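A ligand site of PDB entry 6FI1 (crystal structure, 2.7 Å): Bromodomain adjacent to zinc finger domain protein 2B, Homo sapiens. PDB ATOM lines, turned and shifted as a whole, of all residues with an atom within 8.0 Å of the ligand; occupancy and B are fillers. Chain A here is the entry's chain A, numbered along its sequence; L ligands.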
ATOM      1  N   ASN A  17     -32.602 -38.497 -16.660  1.00  0.00           N
ATOM      2  CA  ASN A  17     -33.169 -37.152 -16.510  1.00  0.00           C
ATOM      3  C   ASN A  17     -32.590 -36.075 -17.420  1.00  0.00           C
ATOM      4  O   ASN A  17     -32.452 -34.930 -17.021  1.00  0.00           O
ATOM      5  CB  ASN A  17     -33.110 -36.701 -15.058  1.00  0.00           C
ATOM      6  CG  ASN A  17     -33.867 -37.627 -14.139  1.00  0.00           C
ATOM      7  OD1 ASN A  17     -33.260 -38.269 -13.280  1.00  0.00           O
ATOM      8  ND2 ASN A  17     -35.196 -37.708 -14.318  1.00  0.00           N
ATOM      9  N   GLU A  18     -32.323 -36.452 -18.655  1.00  0.00           N
ATOM     10  CA  GLU A  18     -31.871 -35.530 -19.687  1.00  0.00           C
ATOM     11  C   GLU A  18     -32.457 -34.092 -19.628  1.00  0.00           C
ATOM     12  O   GLU A  18     -31.725 -33.136 -19.829  1.00  0.00           O
ATOM     13  CB  GLU A  18     -32.077 -36.170 -21.081  1.00  0.00           C
ATOM     14  CG  GLU A  18     -30.912 -37.073 -21.508  1.00  0.00           C
ATOM     15  CD  GLU A  18     -31.244 -38.065 -22.645  1.00  0.00           C
ATOM     16  OE1 GLU A  18     -30.613 -37.975 -23.739  1.00  0.00           O
ATOM     17  OE2 GLU A  18     -32.123 -38.942 -22.440  1.00  0.00           O
ATOM     18  N   GLU A  19     -33.744 -33.921 -19.334  1.00  0.00           N
ATOM     19  CA  GLU A  19     -34.295 -32.557 -19.172  1.00  0.00           C
ATOM     20  C   GLU A  19     -33.635 -31.698 -18.062  1.00  0.00           C
ATOM     21  O   GLU A  19     -33.661 -30.459 -18.119  1.00  0.00           O
ATOM     22  CB  GLU A  19     -35.819 -32.555 -18.948  1.00  0.00           C
ATOM     23  CG  GLU A  19     -36.324 -31.119 -18.715  1.00  0.00           C
ATOM     24  CD  GLU A  19     -37.810 -30.912 -18.788  1.00  0.00           C
ATOM     25  OE1 GLU A  19     -38.533 -31.809 -19.265  1.00  0.00           O
ATOM     26  OE2 GLU A  19     -38.238 -29.821 -18.351  1.00  0.00           O
ATOM     27  N   LEU A  20     -33.079 -32.331 -17.036  1.00  0.00           N
ATOM     28  CA  LEU A  20     -32.370 -31.574 -15.992  1.00  0.00           C
ATOM     29  C   LEU A  20     -30.859 -31.687 -16.087  1.00  0.00           C
ATOM     30  O   LEU A  20     -30.149 -31.394 -15.132  1.00  0.00           O
ATOM     31  CB  LEU A  20     -32.839 -32.058 -14.627  1.00  0.00           C
ATOM     32  CG  LEU A  20     -34.305 -31.887 -14.260  1.00  0.00           C
ATOM     33  CD1 LEU A  20     -34.483 -32.473 -12.875  1.00  0.00           C
ATOM     34  CD2 LEU A  20     -34.787 -30.436 -14.296  1.00  0.00           C
ATOM     35  N   LEU A  21     -30.358 -32.096 -17.239  1.00  0.00           N
ATOM     36  CA  LEU A  21     -28.960 -32.369 -17.416  1.00  0.00           C
ATOM     37  C   LEU A  21     -28.359 -31.216 -18.168  1.00  0.00           C
ATOM     38  O   LEU A  21     -28.651 -31.021 -19.332  1.00  0.00           O
ATOM     39  CB  LEU A  21     -28.763 -33.687 -18.163  1.00  0.00           C
ATOM     40  CG  LEU A  21     -27.343 -34.298 -18.222  1.00  0.00           C
ATOM     41  CD1 LEU A  21     -26.620 -34.502 -16.882  1.00  0.00           C
ATOM     42  CD2 LEU A  21     -27.414 -35.650 -18.917  1.00  0.00           C
ATOM     43  N   LEU A  22     -27.551 -30.408 -17.499  1.00  0.00           N
ATOM     44  CA  LEU A  22     -26.903 -29.294 -18.168  1.00  0.00           C
ATOM     45  C   LEU A  22     -25.622 -29.730 -18.860  1.00  0.00           C
ATOM     46  O   LEU A  22     -24.675 -30.132 -18.201  1.00  0.00           O
ATOM     47  CB  LEU A  22     -26.578 -28.212 -17.149  1.00  0.00           C
ATOM     48  CG  LEU A  22     -27.752 -27.724 -16.325  1.00  0.00           C
ATOM     49  CD1 LEU A  22     -27.265 -26.618 -15.395  1.00  0.00           C
ATOM     50  CD2 LEU A  22     -28.919 -27.238 -17.168  1.00  0.00           C
ATOM     51  N   LEU A  23     -25.616 -29.682 -20.201  1.00  0.00           N
ATOM     52  CA  LEU A  23     -24.398 -29.860 -20.995  1.00  0.00           C
ATOM     53  C   LEU A  23     -23.681 -28.512 -21.035  1.00  0.00           C
ATOM     54  O   LEU A  23     -24.253 -27.537 -21.494  1.00  0.00           O
ATOM     55  CB  LEU A  23     -24.750 -30.300 -22.432  1.00  0.00           C
ATOM     56  CG  LEU A  23     -23.658 -30.916 -23.337  1.00  0.00           C
ATOM     57  CD1 LEU A  23     -24.308 -31.817 -24.391  1.00  0.00           C
ATOM     58  CD2 LEU A  23     -22.765 -29.893 -24.054  1.00  0.00           C
ATOM     59  N   CYS A  24     -22.441 -28.453 -20.557  1.00  0.00           N
ATOM     60  CA  CYS A  24     -21.683 -27.196 -20.606  1.00  0.00           C
ATOM     61  C   CYS A  24     -21.195 -26.964 -22.017  1.00  0.00           C
ATOM     62  O   CYS A  24     -20.502 -27.797 -22.564  1.00  0.00           O
ATOM     63  CB  CYS A  24     -20.512 -27.181 -19.624  1.00  0.00           C
ATOM     64  SG  CYS A  24     -19.265 -25.936 -20.055  1.00  0.00           S
ATOM     65  N   ASP A  25     -21.510 -25.800 -22.597  1.00  0.00           N
ATOM     66  CA  ASP A  25     -21.071 -25.510 -23.969  1.00  0.00           C
ATOM     67  C   ASP A  25     -19.634 -25.074 -24.128  1.00  0.00           C
ATOM     68  O   ASP A  25     -19.185 -24.892 -25.259  1.00  0.00           O
ATOM     69  CB  ASP A  25     -21.985 -24.475 -24.608  1.00  0.00           C
ATOM     70  CG  ASP A  25     -23.350 -25.032 -24.858  1.00  0.00           C
ATOM     71  OD1 ASP A  25     -23.488 -25.872 -25.793  1.00  0.00           O
ATOM     72  OD2 ASP A  25     -24.261 -24.652 -24.110  1.00  0.00           O
ATOM     73  N   GLY A  26     -18.924 -24.889 -23.016  1.00  0.00           N
ATOM     74  CA  GLY A  26     -17.484 -24.738 -23.030  1.00  0.00           C
ATOM     75  C   GLY A  26     -16.798 -26.056 -23.318  1.00  0.00           C
ATOM     76  O   GLY A  26     -16.233 -26.254 -24.403  1.00  0.00           O
ATOM     77  N   ASP A  28     -18.212 -29.285 -23.060  1.00  0.00           N
ATOM     78  CA  ASP A  28     -19.128 -30.397 -23.343  1.00  0.00           C
ATOM     79  C   ASP A  28     -19.448 -31.325 -22.183  1.00  0.00           C
ATOM     80  O   ASP A  28     -19.932 -32.405 -22.439  1.00  0.00           O
ATOM     81  CB  ASP A  28     -18.656 -31.206 -24.567  1.00  0.00           C
ATOM     82  CG  ASP A  28     -18.912 -30.484 -25.888  1.00  0.00           C
ATOM     83  OD1 ASP A  28     -19.794 -29.583 -25.915  1.00  0.00           O
ATOM     84  OD2 ASP A  28     -18.245 -30.838 -26.891  1.00  0.00           O
ATOM     85  N   LYS A  29     -19.258 -30.908 -20.934  1.00  0.00           N
ATOM     86  CA  LYS A  29     -19.533 -31.793 -19.789  1.00  0.00           C
ATOM     87  C   LYS A  29     -20.916 -31.562 -19.269  1.00  0.00           C
ATOM     88  O   LYS A  29     -21.485 -30.527 -19.470  1.00  0.00           O
ATOM     89  CB  LYS A  29     -18.583 -31.563 -18.629  1.00  0.00           C
ATOM     90  CG  LYS A  29     -17.224 -32.207 -18.733  1.00  0.00           C
ATOM     91  CD  LYS A  29     -16.445 -31.856 -17.474  1.00  0.00           C
ATOM     92  CE  LYS A  29     -15.037 -32.419 -17.511  1.00  0.00           C
ATOM     93  NZ  LYS A  29     -14.118 -31.549 -18.311  1.00  0.00           N
ATOM     94  N   GLY A  30     -21.406 -32.511 -18.505  1.00  0.00           N
ATOM     95  CA  GLY A  30     -22.786 -32.566 -18.085  1.00  0.00           C
ATOM     96  C   GLY A  30     -22.828 -32.526 -16.593  1.00  0.00           C
ATOM     97  O   GLY A  30     -21.881 -32.906 -15.936  1.00  0.00           O
ATOM     98  N   CYS A  31     -23.905 -31.976 -16.077  1.00  0.00           N
ATOM     99  CA  CYS A  31     -24.183 -32.030 -14.674  1.00  0.00           C
ATOM    100  C   CYS A  31     -25.697 -31.825 -14.444  1.00  0.00           C
ATOM    101  O   CYS A  31     -26.265 -30.878 -14.913  1.00  0.00           O
ATOM    102  CB  CYS A  31     -23.377 -30.981 -13.932  1.00  0.00           C
ATOM    103  SG  CYS A  31     -23.454 -31.323 -12.189  1.00  0.00           S
ATOM    104  N   THR A  33     -28.972 -30.604 -12.690  1.00  0.00           N
ATOM    105  CA  THR A  33     -29.241 -29.421 -11.894  1.00  0.00           C
ATOM    106  C   THR A  33     -29.252 -29.794 -10.401  1.00  0.00           C
ATOM    107  O   THR A  33     -28.786 -29.064  -9.528  1.00  0.00           O
ATOM    108  CB  THR A  33     -30.614 -28.806 -12.246  1.00  0.00           C
ATOM    109  OG1 THR A  33     -31.590 -29.832 -12.311  1.00  0.00           O
ATOM    110  CG2 THR A  33     -30.604 -28.105 -13.544  1.00  0.00           C
ATOM    111  N   THR A  42     -33.282 -22.668 -11.726  1.00  0.00           N
ATOM    112  CA  THR A  42     -33.633 -22.154 -13.078  1.00  0.00           C
ATOM    113  C   THR A  42     -33.015 -23.017 -14.198  1.00  0.00           C
ATOM    114  O   THR A  42     -31.786 -22.956 -14.425  1.00  0.00           O
ATOM    115  CB  THR A  42     -33.146 -20.703 -13.290  1.00  0.00           C
ATOM    116  OG1 THR A  42     -33.821 -19.815 -12.380  1.00  0.00           O
ATOM    117  CG2 THR A  42     -33.384 -20.217 -14.746  1.00  0.00           C
ATOM    118  N   ILE A  43     -33.849 -23.779 -14.905  1.00  0.00           N
ATOM    119  CA  ILE A  43     -33.369 -24.520 -16.086  1.00  0.00           C
ATOM    120  C   ILE A  43     -33.008 -23.419 -17.118  1.00  0.00           C
ATOM    121  O   ILE A  43     -33.883 -22.652 -17.544  1.00  0.00           O
ATOM    122  CB  ILE A  43     -34.414 -25.524 -16.665  1.00  0.00           C
ATOM    123  CG1 ILE A  43     -34.910 -26.527 -15.625  1.00  0.00           C
ATOM    124  CG2 ILE A  43     -33.818 -26.318 -17.816  1.00  0.00           C
ATOM    125  CD1 ILE A  43     -36.128 -27.314 -16.061  1.00  0.00           C
ATOM    126  N   PRO A  44     -31.717 -23.327 -17.511  1.00  0.00           N
ATOM    127  CA  PRO A  44     -31.223 -22.169 -18.258  1.00  0.00           C
ATOM    128  C   PRO A  44     -31.985 -21.965 -19.547  1.00  0.00           C
ATOM    129  O   PRO A  44     -32.379 -22.939 -20.191  1.00  0.00           O
ATOM    130  CB  PRO A  44     -29.777 -22.549 -18.590  1.00  0.00           C
ATOM    131  CG  PRO A  44     -29.825 -24.029 -18.703  1.00  0.00           C
ATOM    132  CD  PRO A  44     -30.785 -24.460 -17.635  1.00  0.00           C
ATOM    133  N   ASP A  45     -32.172 -20.722 -19.918  1.00  0.00           N
ATOM    134  CA  ASP A  45     -32.991 -20.399 -21.061  1.00  0.00           C
ATOM    135  C   ASP A  45     -32.262 -20.657 -22.383  1.00  0.00           C
ATOM    136  O   ASP A  45     -32.906 -21.009 -23.394  1.00  0.00           O
ATOM    137  CB  ASP A  45     -33.442 -18.956 -20.977  1.00  0.00           C
ATOM    138  CG  ASP A  45     -34.635 -18.693 -21.805  1.00  0.00           C
ATOM    139  OD1 ASP A  45     -35.741 -19.100 -21.383  1.00  0.00           O
ATOM    140  OD2 ASP A  45     -34.460 -18.110 -22.889  1.00  0.00           O
ATOM    141  N   GLY A  46     -30.936 -20.499 -22.356  1.00  0.00           N
ATOM    142  CA  GLY A  46     -30.079 -20.661 -23.526  1.00  0.00           C
ATOM    143  C   GLY A  46     -28.870 -21.491 -23.183  1.00  0.00           C
ATOM    144  O   GLY A  46     -29.017 -22.688 -22.883  1.00  0.00           O
ATOM    145  N   ASP A  47     -27.691 -20.851 -23.178  1.00  0.00           N
ATOM    146  CA  ASP A  47     -26.390 -21.519 -23.086  1.00  0.00           C
ATOM    147  C   ASP A  47     -25.749 -21.595 -21.678  1.00  0.00           C
ATOM    148  O   ASP A  47     -25.770 -20.637 -20.916  1.00  0.00           O
ATOM    149  CB  ASP A  47     -25.385 -20.884 -24.065  1.00  0.00           C
ATOM    150  CG  ASP A  47     -25.528 -21.436 -25.488  1.00  0.00           C
ATOM    151  OD1 ASP A  47     -25.375 -22.666 -25.679  1.00  0.00           O
ATOM    152  OD2 ASP A  47     -25.819 -20.648 -26.411  1.00  0.00           O
ATOM    153  N   TRP A  48     -25.129 -22.742 -21.399  1.00  0.00           N
ATOM    154  CA  TRP A  48     -24.621 -23.073 -20.076  1.00  0.00           C
ATOM    155  C   TRP A  48     -23.088 -23.146 -20.052  1.00  0.00           C
ATOM    156  O   TRP A  48     -22.460 -23.951 -20.739  1.00  0.00           O
ATOM    157  CB  TRP A  48     -25.204 -24.419 -19.643  1.00  0.00           C
ATOM    158  CG  TRP A  48     -24.686 -24.909 -18.339  1.00  0.00           C
ATOM    159  CD1 TRP A  48     -24.005 -26.067 -18.076  1.00  0.00           C
ATOM    160  CD2 TRP A  48     -24.822 -24.239 -17.111  1.00  0.00           C
ATOM    161  NE1 TRP A  48     -23.692 -26.147 -16.747  1.00  0.00           N
ATOM    162  CE2 TRP A  48     -24.191 -25.025 -16.136  1.00  0.00           C
ATOM    163  CE3 TRP A  48     -25.420 -23.036 -16.741  1.00  0.00           C
ATOM    164  CZ2 TRP A  48     -24.134 -24.637 -14.809  1.00  0.00           C
ATOM    165  CZ3 TRP A  48     -25.380 -22.661 -15.438  1.00  0.00           C
ATOM    166  CH2 TRP A  48     -24.757 -23.449 -14.481  1.00  0.00           C
ATOM    167  N   PHE A  49     -22.478 -22.308 -19.249  1.00  0.00           N
ATOM    168  CA  PHE A  49     -21.080 -22.453 -18.998  1.00  0.00           C
ATOM    169  C   PHE A  49     -20.927 -22.921 -17.570  1.00  0.00           C
ATOM    170  O   PHE A  49     -21.476 -22.312 -16.641  1.00  0.00           O
ATOM    171  CB  PHE A  49     -20.383 -21.170 -19.299  1.00  0.00           C
ATOM    172  CG  PHE A  49     -20.440 -20.812 -20.758  1.00  0.00           C
ATOM    173  CD1 PHE A  49     -19.541 -21.377 -21.668  1.00  0.00           C
ATOM    174  CD2 PHE A  49     -21.428 -19.945 -21.243  1.00  0.00           C
ATOM    175  CE1 PHE A  49     -19.608 -21.048 -23.019  1.00  0.00           C
ATOM    176  CE2 PHE A  49     -21.486 -19.628 -22.586  1.00  0.00           C
ATOM    177  CZ  PHE A  49     -20.575 -20.182 -23.480  1.00  0.00           C
HETATM  178  C1  LIG L   1     -30.666 -26.875 -21.335  1.00  0.00           C
HETATM  179  C2  LIG L   1     -30.643 -28.097 -20.635  1.00  0.00           C
HETATM  180  C3  LIG L   1     -31.824 -28.726 -20.229  1.00  0.00           C
HETATM  181  C4  LIG L   1     -28.313 -26.644 -21.810  1.00  0.00           C
HETATM  182  C5  LIG L   1     -27.307 -25.634 -22.412  1.00  0.00           C
HETATM  183  N1  LIG L   1     -29.597 -26.175 -21.786  1.00  0.00           N
HETATM  184  N2  LIG L   1     -26.153 -26.320 -23.026  1.00  0.00           N
HETATM  185  C6  LIG L   1     -31.916 -26.304 -21.618  1.00  0.00           C
HETATM  186  N3  LIG L   1     -34.200 -28.686 -20.143  1.00  0.00           N
HETATM  187  C7  LIG L   1     -33.097 -26.919 -21.203  1.00  0.00           C
HETATM  188  C8  LIG L   1     -33.062 -28.130 -20.520  1.00  0.00           C
HETATM  189  O1  LIG L   1     -27.916 -27.747 -21.420  1.00  0.00           O
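The backbone carbonyl oxygen (O) of Trp 48 sits at hydrogen-bond distance from the backbone NH (N) of Asp 25 (2.8 Å). The backbone carbonyl oxygen of Leu 22 is in hydrogen-bond range of the backbone NH of Cys 31 (2.9 Å).
An oxygen (O1) of the ligand is in hydrogen-bond range of the backbone NH of Leu 23, 3.2 Å away. O of Leu 23 lies within hydrogen-bond range of N2 of the ligand, at 2.7 Å. A nitrogen (N3) of the ligand sits at hydrogen-bond distance from the backbone carbonyl oxygen of Glu 19 (2.7 Å). A nitrogen (N2) of the ligand lies within salt-bridge range of the side-chain carboxylate (OD2) of Asp 25 (2.7 Å).
Leu 21 touches the ligand (O to C2, 3.8 Å). CA of Leu 22 touches O1 of the ligand (3.7 Å). Ile 43 touches the ligand (CG2 to C8, 3.3 Å). O of Pro 44 touches C6 of the ligand, 3.7 Å away. O of Gly 46 touches C5 of the ligand (3.4 Å). Trp 48 touches the ligand (CB to C5, 3.7 Å). Hydrophobic or aromatic side chains within 4 Å of the ligand: Leu 22, Ile 43, Pro 44 and Trp 48. Nine residues have an atom within 4 Å of the ligand: Glu 19, Leu 21, Leu 22, Leu 23, Asp 25, Ile 43, Pro 44, Gly 46 and Trp 48. Along chain A the residues within 4 Å of the ligand span positions 19 to 48. The nearest printed residue that does not touch the ligand is Asp 47 (4.3 Å).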
